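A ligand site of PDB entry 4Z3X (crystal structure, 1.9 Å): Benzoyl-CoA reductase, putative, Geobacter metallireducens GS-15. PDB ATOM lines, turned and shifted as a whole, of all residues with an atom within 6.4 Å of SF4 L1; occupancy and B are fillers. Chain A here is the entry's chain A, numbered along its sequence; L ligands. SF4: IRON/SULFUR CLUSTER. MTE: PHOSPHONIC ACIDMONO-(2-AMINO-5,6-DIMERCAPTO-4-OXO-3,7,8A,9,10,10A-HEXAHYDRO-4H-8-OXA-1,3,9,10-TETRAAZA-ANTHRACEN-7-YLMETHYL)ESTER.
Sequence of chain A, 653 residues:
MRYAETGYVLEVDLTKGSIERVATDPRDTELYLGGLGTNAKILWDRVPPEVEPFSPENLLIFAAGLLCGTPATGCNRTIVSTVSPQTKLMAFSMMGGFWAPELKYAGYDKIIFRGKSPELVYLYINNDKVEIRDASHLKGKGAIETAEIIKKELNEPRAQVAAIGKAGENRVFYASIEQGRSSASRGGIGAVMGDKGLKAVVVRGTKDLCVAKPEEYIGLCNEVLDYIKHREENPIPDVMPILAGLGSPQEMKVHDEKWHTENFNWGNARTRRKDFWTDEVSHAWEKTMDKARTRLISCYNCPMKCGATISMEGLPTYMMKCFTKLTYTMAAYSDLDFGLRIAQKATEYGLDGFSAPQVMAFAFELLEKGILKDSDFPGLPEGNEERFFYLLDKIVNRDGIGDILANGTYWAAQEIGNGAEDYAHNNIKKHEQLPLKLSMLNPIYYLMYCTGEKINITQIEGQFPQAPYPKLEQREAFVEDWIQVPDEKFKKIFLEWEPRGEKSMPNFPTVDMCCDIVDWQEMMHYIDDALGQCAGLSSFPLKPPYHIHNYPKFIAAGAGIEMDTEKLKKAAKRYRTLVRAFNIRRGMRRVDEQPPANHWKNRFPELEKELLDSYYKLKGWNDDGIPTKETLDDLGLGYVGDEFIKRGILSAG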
ATOM      1  N   GLY A  74     -26.221  19.688   5.123  1.00  0.00           N
ATOM      2  CA  GLY A  74     -26.250  18.355   5.702  1.00  0.00           C
ATOM      3  C   GLY A  74     -26.979  17.280   4.865  1.00  0.00           C
ATOM      4  O   GLY A  74     -27.224  16.187   5.370  1.00  0.00           O
ATOM      5  N   CYS A  75     -27.320  17.542   3.601  1.00  0.00           N
ATOM      6  CA  CYS A  75     -27.966  16.509   2.795  1.00  0.00           C
ATOM      7  C   CYS A  75     -26.909  15.691   2.026  1.00  0.00           C
ATOM      8  O   CYS A  75     -26.479  16.056   0.933  1.00  0.00           O
ATOM      9  CB  CYS A  75     -29.001  17.140   1.841  1.00  0.00           C
ATOM     10  SG  CYS A  75     -30.028  15.882   1.010  1.00  0.00           S
ATOM     11  N   ASN A  76     -26.428  14.616   2.622  1.00  0.00           N
ATOM     12  CA  ASN A  76     -25.237  13.946   2.122  1.00  0.00           C
ATOM     13  C   ASN A  76     -25.241  12.440   2.360  1.00  0.00           C
ATOM     14  O   ASN A  76     -24.179  11.787   2.270  1.00  0.00           O
ATOM     15  CB  ASN A  76     -24.016  14.603   2.820  1.00  0.00           C
ATOM     16  CG  ASN A  76     -24.208  14.649   4.342  1.00  0.00           C
ATOM     17  OD1 ASN A  76     -24.794  13.751   4.872  1.00  0.00           O
ATOM     18  ND2 ASN A  76     -23.746  15.715   5.021  1.00  0.00           N
ATOM     19  N   ARG A  77     -26.406  11.843   2.659  1.00  0.00           N
ATOM     20  CA  ARG A  77     -26.385  10.437   3.082  1.00  0.00           C
ATOM     21  C   ARG A  77     -26.448   9.461   1.917  1.00  0.00           C
ATOM     22  O   ARG A  77     -27.163   9.660   0.943  1.00  0.00           O
ATOM     23  CB  ARG A  77     -27.535  10.105   4.080  1.00  0.00           C
ATOM     24  CG  ARG A  77     -27.022   9.899   5.512  1.00  0.00           C
ATOM     25  CD  ARG A  77     -26.544  11.236   6.208  1.00  0.00           C
ATOM     26  NE  ARG A  77     -25.861  10.878   7.454  1.00  0.00           N
ATOM     27  CZ  ARG A  77     -25.033  11.641   8.167  1.00  0.00           C
ATOM     28  NH1 ARG A  77     -24.680  12.887   7.773  1.00  0.00           N
ATOM     29  NH2 ARG A  77     -24.504  11.119   9.276  1.00  0.00           N
ATOM     30  N   GLY A  96     -23.098   8.820   6.267  1.00  0.00           N
ATOM     31  CA  GLY A  96     -22.925  10.235   6.017  1.00  0.00           C
ATOM     32  C   GLY A  96     -21.625  10.562   5.266  1.00  0.00           C
ATOM     33  O   GLY A  96     -21.202   9.827   4.399  1.00  0.00           O
ATOM     34  N   GLY A  97     -21.005  11.688   5.592  1.00  0.00           N
ATOM     35  CA  GLY A  97     -19.720  12.049   4.970  1.00  0.00           C
ATOM     36  C   GLY A  97     -19.864  12.697   3.609  1.00  0.00           C
ATOM     37  O   GLY A  97     -20.618  13.690   3.433  1.00  0.00           O
ATOM     38  N   ARG A 181     -15.151   9.535   8.076  1.00  0.00           N
ATOM     39  CA  ARG A 181     -15.801   9.607   9.404  1.00  0.00           C
ATOM     40  C   ARG A 181     -17.272   9.072   9.353  1.00  0.00           C
ATOM     41  O   ARG A 181     -18.147   9.500  10.150  1.00  0.00           O
ATOM     42  CB  ARG A 181     -15.815  11.056   9.972  1.00  0.00           C
ATOM     43  CG  ARG A 181     -16.601  12.074   9.119  1.00  0.00           C
ATOM     44  CD  ARG A 181     -17.292  13.096  10.009  1.00  0.00           C
ATOM     45  NE  ARG A 181     -18.488  12.432  10.593  1.00  0.00           N
ATOM     46  CZ  ARG A 181     -19.466  13.050  11.243  1.00  0.00           C
ATOM     47  NH1 ARG A 181     -19.396  14.360  11.461  1.00  0.00           N
ATOM     48  NH2 ARG A 181     -20.495  12.321  11.723  1.00  0.00           N
ATOM     49  N   LEU A 246     -28.922  20.564  17.897  1.00  0.00           N
ATOM     50  CA  LEU A 246     -28.947  19.853  16.608  1.00  0.00           C
ATOM     51  C   LEU A 246     -27.772  18.879  16.459  1.00  0.00           C
ATOM     52  O   LEU A 246     -26.805  18.898  17.225  1.00  0.00           O
ATOM     53  CB  LEU A 246     -28.969  20.863  15.458  1.00  0.00           C
ATOM     54  CG  LEU A 246     -30.152  21.844  15.464  1.00  0.00           C
ATOM     55  CD1 LEU A 246     -30.089  22.827  14.284  1.00  0.00           C
ATOM     56  CD2 LEU A 246     -31.470  21.038  15.425  1.00  0.00           C
ATOM     57  N   GLY A 247     -27.869  17.997  15.474  1.00  0.00           N
ATOM     58  CA  GLY A 247     -26.793  17.080  15.135  1.00  0.00           C
ATOM     59  C   GLY A 247     -27.059  15.666  15.626  1.00  0.00           C
ATOM     60  O   GLY A 247     -27.997  15.457  16.386  1.00  0.00           O
ATOM     61  N   SER A 248     -26.215  14.696  15.228  1.00  0.00           N
ATOM     62  CA  SER A 248     -26.176  13.392  15.915  1.00  0.00           C
ATOM     63  C   SER A 248     -25.846  13.637  17.387  1.00  0.00           C
ATOM     64  O   SER A 248     -25.353  14.717  17.706  1.00  0.00           O
ATOM     65  CB  SER A 248     -25.142  12.466  15.280  1.00  0.00           C
ATOM     66  OG  SER A 248     -25.343  12.308  13.860  1.00  0.00           O
ATOM     67  N   GLN A 250     -24.205  14.606  20.499  1.00  0.00           N
ATOM     68  CA  GLN A 250     -22.959  15.358  20.494  1.00  0.00           C
ATOM     69  C   GLN A 250     -21.958  14.812  21.528  1.00  0.00           C
ATOM     70  O   GLN A 250     -21.400  15.574  22.331  1.00  0.00           O
ATOM     71  CB  GLN A 250     -23.300  16.835  20.751  1.00  0.00           C
ATOM     72  CG  GLN A 250     -24.121  17.441  19.572  1.00  0.00           C
ATOM     73  CD  GLN A 250     -23.204  17.756  18.375  1.00  0.00           C
ATOM     74  OE1 GLN A 250     -22.010  17.504  18.448  1.00  0.00           O
ATOM     75  NE2 GLN A 250     -23.753  18.343  17.325  1.00  0.00           N
ATOM     76  N   ILE A 297     -15.017  17.350  13.370  1.00  0.00           N
ATOM     77  CA  ILE A 297     -15.152  17.520  11.911  1.00  0.00           C
ATOM     78  C   ILE A 297     -16.552  17.243  11.384  1.00  0.00           C
ATOM     79  O   ILE A 297     -17.289  16.445  11.935  1.00  0.00           O
ATOM     80  CB  ILE A 297     -14.135  16.624  11.206  1.00  0.00           C
ATOM     81  CG1 ILE A 297     -14.201  15.191  11.734  1.00  0.00           C
ATOM     82  CG2 ILE A 297     -12.643  17.164  11.472  1.00  0.00           C
ATOM     83  CD1 ILE A 297     -13.564  14.159  10.789  1.00  0.00           C
ATOM     84  N   SER A 298     -16.924  17.912  10.305  1.00  0.00           N
ATOM     85  CA  SER A 298     -18.266  17.761   9.797  1.00  0.00           C
ATOM     86  C   SER A 298     -18.386  16.729   8.645  1.00  0.00           C
ATOM     87  O   SER A 298     -17.400  16.397   7.970  1.00  0.00           O
ATOM     88  CB  SER A 298     -18.790  19.111   9.299  1.00  0.00           C
ATOM     89  OG  SER A 298     -18.906  20.116  10.301  1.00  0.00           O
ATOM     90  N   CYS A 299     -19.601  16.256   8.378  1.00  0.00           N
ATOM     91  CA  CYS A 299     -19.897  15.716   7.027  1.00  0.00           C
ATOM     92  C   CYS A 299     -19.960  16.852   5.987  1.00  0.00           C
ATOM     93  O   CYS A 299     -19.697  18.024   6.321  1.00  0.00           O
ATOM     94  CB  CYS A 299     -21.246  14.953   7.066  1.00  0.00           C
ATOM     95  SG  CYS A 299     -21.219  13.767   8.334  1.00  0.00           S
ATOM     96  N   TYR A 300     -20.270  16.490   4.745  1.00  0.00           N
ATOM     97  CA  TYR A 300     -20.359  17.429   3.620  1.00  0.00           C
ATOM     98  C   TYR A 300     -21.394  18.477   3.821  1.00  0.00           C
ATOM     99  O   TYR A 300     -22.516  18.159   4.161  1.00  0.00           O
ATOM    100  CB  TYR A 300     -20.685  16.697   2.340  1.00  0.00           C
ATOM    101  CG  TYR A 300     -20.664  17.539   1.091  1.00  0.00           C
ATOM    102  CD1 TYR A 300     -19.483  18.185   0.683  1.00  0.00           C
ATOM    103  CD2 TYR A 300     -21.801  17.677   0.277  1.00  0.00           C
ATOM    104  CE1 TYR A 300     -19.422  18.925  -0.470  1.00  0.00           C
ATOM    105  CE2 TYR A 300     -21.756  18.426  -0.926  1.00  0.00           C
ATOM    106  CZ  TYR A 300     -20.548  19.043  -1.277  1.00  0.00           C
ATOM    107  OH  TYR A 300     -20.432  19.769  -2.461  1.00  0.00           O
ATOM    108  N   ASN A 301     -21.000  19.738   3.624  1.00  0.00           N
ATOM    109  CA  ASN A 301     -21.891  20.899   3.680  1.00  0.00           C
ATOM    110  C   ASN A 301     -22.739  20.947   4.997  1.00  0.00           C
ATOM    111  O   ASN A 301     -23.929  21.217   4.975  1.00  0.00           O
ATOM    112  CB  ASN A 301     -22.793  20.868   2.435  1.00  0.00           C
ATOM    113  CG  ASN A 301     -23.552  22.167   2.241  1.00  0.00           C
ATOM    114  OD1 ASN A 301     -23.085  23.248   2.637  1.00  0.00           O
ATOM    115  ND2 ASN A 301     -24.749  22.084   1.630  1.00  0.00           N
ATOM    116  N   CYS A 302     -22.062  20.786   6.133  1.00  0.00           N
ATOM    117  CA  CYS A 302     -22.688  20.969   7.420  1.00  0.00           C
ATOM    118  C   CYS A 302     -21.825  21.630   8.499  1.00  0.00           C
ATOM    119  O   CYS A 302     -20.660  21.227   8.703  1.00  0.00           O
ATOM    120  CB  CYS A 302     -23.153  19.599   7.946  1.00  0.00           C
ATOM    121  SG  CYS A 302     -24.124  19.704   9.447  1.00  0.00           S
ATOM    122  N   PRO A 303     -22.419  22.538   9.306  1.00  0.00           N
ATOM    123  CA  PRO A 303     -21.602  23.212  10.340  1.00  0.00           C
ATOM    124  C   PRO A 303     -21.554  22.514  11.689  1.00  0.00           C
ATOM    125  O   PRO A 303     -20.759  22.919  12.541  1.00  0.00           O
ATOM    126  CB  PRO A 303     -22.293  24.573  10.454  1.00  0.00           C
ATOM    127  CG  PRO A 303     -23.769  24.207  10.292  1.00  0.00           C
ATOM    128  CD  PRO A 303     -23.688  23.245   9.083  1.00  0.00           C
ATOM    129  N   MET A 304     -22.349  21.458  11.892  1.00  0.00           N
ATOM    130  CA  MET A 304     -22.468  20.875  13.206  1.00  0.00           C
ATOM    131  C   MET A 304     -21.252  20.081  13.767  1.00  0.00           C
ATOM    132  O   MET A 304     -21.219  19.853  14.951  1.00  0.00           O
ATOM    133  CB  MET A 304     -23.687  19.927  13.202  1.00  0.00           C
ATOM    134  CG  MET A 304     -25.032  20.639  13.029  1.00  0.00           C
ATOM    135  SD  MET A 304     -25.302  22.177  13.894  1.00  0.00           S
ATOM    136  CE  MET A 304     -25.022  21.702  15.596  1.00  0.00           C
ATOM    137  N   LYS A 305     -20.357  19.595  12.905  1.00  0.00           N
ATOM    138  CA  LYS A 305     -19.125  18.873  13.337  1.00  0.00           C
ATOM    139  C   LYS A 305     -19.313  17.920  14.537  1.00  0.00           C
ATOM    140  O   LYS A 305     -18.597  17.995  15.577  1.00  0.00           O
ATOM    141  CB  LYS A 305     -17.934  19.899  13.578  1.00  0.00           C
ATOM    142  CG  LYS A 305     -18.201  21.041  14.554  1.00  0.00           C
ATOM    143  CD  LYS A 305     -17.010  22.080  14.674  1.00  0.00           C
ATOM    144  CE  LYS A 305     -17.372  23.150  15.766  1.00  0.00           C
ATOM    145  NZ  LYS A 305     -16.395  24.243  15.857  1.00  0.00           N
ATOM    146  N   CYS A 306     -20.241  16.943  14.350  1.00  0.00           N
ATOM    147  CA  CYS A 306     -20.566  15.932  15.336  1.00  0.00           C
ATOM    148  C   CYS A 306     -19.451  14.912  15.556  1.00  0.00           C
ATOM    149  O   CYS A 306     -19.336  14.319  16.632  1.00  0.00           O
ATOM    150  CB  CYS A 306     -21.851  15.171  14.883  1.00  0.00           C
ATOM    151  SG  CYS A 306     -23.174  16.323  14.497  1.00  0.00           S
ATOM    152  N   GLY A 307     -18.634  14.697  14.532  1.00  0.00           N
ATOM    153  CA  GLY A 307     -17.624  13.655  14.592  1.00  0.00           C
ATOM    154  C   GLY A 307     -16.262  14.155  14.994  1.00  0.00           C
ATOM    155  O   GLY A 307     -16.044  15.354  15.134  1.00  0.00           O
ATOM    156  N   LYS A 321     -18.100   9.054  15.843  1.00  0.00           N
ATOM    157  CA  LYS A 321     -19.160   9.934  16.366  1.00  0.00           C
ATOM    158  C   LYS A 321     -20.150   9.099  17.192  1.00  0.00           C
ATOM    159  O   LYS A 321     -20.120   7.846  17.142  1.00  0.00           O
ATOM    160  CB  LYS A 321     -19.902  10.645  15.215  1.00  0.00           C
ATOM    161  CG  LYS A 321     -21.026   9.844  14.581  1.00  0.00           C
ATOM    162  CD  LYS A 321     -20.613   8.416  14.034  1.00  0.00           C
ATOM    163  CE  LYS A 321     -19.757   8.519  12.720  1.00  0.00           C
ATOM    164  NZ  LYS A 321     -19.522   7.226  12.009  1.00  0.00           N
ATOM    165  N   CYS A 534     -29.307  14.392   6.479  1.00  0.00           N
ATOM    166  CA  CYS A 534     -28.881  13.901   7.802  1.00  0.00           C
ATOM    167  C   CYS A 534     -30.025  14.073   8.809  1.00  0.00           C
ATOM    168  O   CYS A 534     -30.529  15.191   8.981  1.00  0.00           O
ATOM    169  CB  CYS A 534     -27.684  14.626   8.366  1.00  0.00           C
ATOM    170  SG  CYS A 534     -27.043  13.789   9.871  1.00  0.00           S
ATOM    171  N   ALA A 535     -30.311  13.008   9.525  1.00  0.00           N
ATOM    172  CA  ALA A 535     -31.308  13.025  10.614  1.00  0.00           C
ATOM    173  C   ALA A 535     -30.879  14.008  11.739  1.00  0.00           C
ATOM    174  O   ALA A 535     -31.734  14.475  12.504  1.00  0.00           O
ATOM    175  CB  ALA A 535     -31.490  11.653  11.135  1.00  0.00           C
ATOM    176  N   GLY A 536     -29.581  14.321  11.798  1.00  0.00           N
ATOM    177  CA  GLY A 536     -29.025  15.341  12.709  1.00  0.00           C
ATOM    178  C   GLY A 536     -29.608  16.729  12.613  1.00  0.00           C
ATOM    179  O   GLY A 536     -29.581  17.506  13.586  1.00  0.00           O
ATOM    180  N   LEU A 537     -30.186  17.050  11.460  1.00  0.00           N
ATOM    181  CA  LEU A 537     -30.875  18.286  11.225  1.00  0.00           C
ATOM    182  C   LEU A 537     -32.357  18.110  10.946  1.00  0.00           C
ATOM    183  O   LEU A 537     -33.035  19.067  10.518  1.00  0.00           O
ATOM    184  CB  LEU A 537     -30.228  19.031  10.045  1.00  0.00           C
ATOM    185  CG  LEU A 537     -28.757  19.377  10.170  1.00  0.00           C
ATOM    186  CD1 LEU A 537     -28.216  20.007   8.831  1.00  0.00           C
ATOM    187  CD2 LEU A 537     -28.486  20.341  11.394  1.00  0.00           C
HETATM  188 FE1  SF4 L   1     -22.607  15.002   9.810  1.00  0.00          FE
HETATM  189 FE2  SF4 L   1     -23.849  17.563  10.098  1.00  0.00          FE
HETATM  190 FE3  SF4 L   1     -23.400  15.952  12.330  1.00  0.00          FE
HETATM  191 FE4  SF4 L   1     -25.188  15.094  10.406  1.00  0.00          FE
HETATM  192  S1  SF4 L   1     -25.325  16.970  11.707  1.00  0.00           S
HETATM  193  S2  SF4 L   1     -23.731  13.807  11.449  1.00  0.00           S
HETATM  194  S3  SF4 L   1     -24.119  15.975   8.566  1.00  0.00           S
HETATM  195  S4  SF4 L   1     -21.898  16.911  10.979  1.00  0.00           S
HETATM  196  N1  MTE L   2     -29.273  10.437   8.942  1.00  0.00           N
HETATM  197  C2  MTE L   2     -30.177   9.670   8.300  1.00  0.00           C
HETATM  198  N2  MTE L   2     -30.825  10.135   7.114  1.00  0.00           N
HETATM  199  N3  MTE L   2     -30.663   8.471   8.792  1.00  0.00           N
HETATM  200  C4  MTE L   2     -30.125   7.921   9.929  1.00  0.00           C
HETATM  201  O4  MTE L   2     -30.610   6.797  10.340  1.00  0.00           O
HETATM  202  N5  MTE L   2     -28.519   8.223  11.833  1.00  0.00           N
HETATM  203  C6  MTE L   2     -27.893   9.339  12.656  1.00  0.00           C
HETATM  204  C7  MTE L   2     -27.036  10.311  11.848  1.00  0.00           C
HETATM  205  N8  MTE L   2     -27.726  10.702  10.640  1.00  0.00           N
HETATM  206  C9  MTE L   2     -29.115   8.701  10.616  1.00  0.00           C
HETATM  207  C10 MTE L   2     -28.703   9.875  10.081  1.00  0.00           C
HETATM  208  C1' MTE L   2     -26.889   8.889  13.902  1.00  0.00           C
HETATM  209  S1' MTE L   2     -27.736   8.358  15.412  1.00  0.00           S
HETATM  210  C2' MTE L   2     -25.713   8.944  13.779  1.00  0.00           C
HETATM  211  S2' MTE L   2     -24.687   8.332  15.039  1.00  0.00           S
HETATM  212  C3' MTE L   2     -25.000   9.342  12.420  1.00  0.00           C
HETATM  213  O3' MTE L   2     -25.918   9.617  11.398  1.00  0.00           O
HETATM  214  C4' MTE L   2     -24.224   8.198  11.829  1.00  0.00           C
HETATM  215  O4' MTE L   2     -23.282   8.702  10.858  1.00  0.00           O
HETATM  216  P   MTE L   2     -22.696   7.687   9.796  1.00  0.00           P
HETATM  217  O1P MTE L   2     -21.621   6.799  10.553  1.00  0.00           O
HETATM  218  O2P MTE L   2     -22.040   8.431   8.631  1.00  0.00           O
HETATM  219  O3P MTE L   2     -23.755   6.875   9.345  1.00  0.00           O
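Merely in contact with SF4 L1: Gly 247, Ser 298 and Met 304.
Hydrophobic or aromatic side chains that line SF4 L1: Met 304.
SG of Cys 302 sits close to N of Met 304 (3.5 Å).
The backbone carbonyl oxygen (O) of Cys 302 sits at hydrogen-bond distance from the side-chain hydroxyl (OG) of Ser 298 (2.6 Å).
The backbone NH (N) of Cys 534 sits at hydrogen-bond distance from the backbone carbonyl oxygen (O) of Gly 74, at 3.0 Å.
The side-chain sulfur (SG) of Cys 299 lies close to the backbone NH (N) of Gly 97, 3.4 Å away.
The guanidinium group (NH1) of Arg 181 is in hydrogen-bond range of the backbone carbonyl oxygen (O) of Ile 297, at 3.0 Å.
The backbone carbonyl oxygen (O) of Gly 74 lies close to the side-chain amide oxygen (OD1) of Asn 76 (3.5 Å).
The side-chain amide nitrogen (ND2) of Asn 76 lies within hydrogen-bond range of the backbone carbonyl oxygen (O) of Tyr 300.
OG of Ser 298 sits at hydrogen-bond distance from N of Lys 305.
A sulfur (S4) of SF4 L1 lies close to the backbone NH of Cys 306 (3.8 Å).
The side-chain sulfur (SG) of Cys 306 is bound to an iron atom (FE3) of SF4 L1 (2.2 Å).
FE2 of SF4 L1 is bound by SG of Cys 302.
An iron atom (FE4) of SF4 L1 is bound by the side-chain sulfur (SG) of Cys 534, at 2.3 Å.
The backbone NH (N) of Cys 299 sits close to a sulfur (S4) of SF4 L1 (3.5 Å).
The side-chain sulfur (SG) of Cys 299 is bound to an iron atom (FE1) of SF4 L1 (2.4 Å).
The guanidinium group of Arg 77 lies close to a sulfur (S3) of SF4 L1 (3.2 Å).
OG of Ser 248 sits close to S2 of SF4 L1.
NH2 of Arg 181 sits close to S2 of SF4 L1 (3.6 Å).
S3 of SF4 L1 sits close to ND2 of Asn 76, 3.6 Å away.
The backbone NH of Lys 305 lies close to a sulfur (S4) of SF4 L1 (3.6 Å).
The side-chain sulfur (SG) of Cys 534 lies close to a nitrogen (N8) of MTE L2 (3.3 Å).
NH2 of Arg 77 lies within salt-bridge range of O2P of MTE L2, at 3.7 Å.
The backbone NH (N) of Ala 535 is in hydrogen-bond range of a nitrogen (N1) of MTE L2 (2.8 Å).
NZ of Lys 321 lies within salt-bridge range of O1P of MTE L2 (2.6 Å).
N of Gly 96 lies within hydrogen-bond range of O2P of MTE L2, at 2.6 Å.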
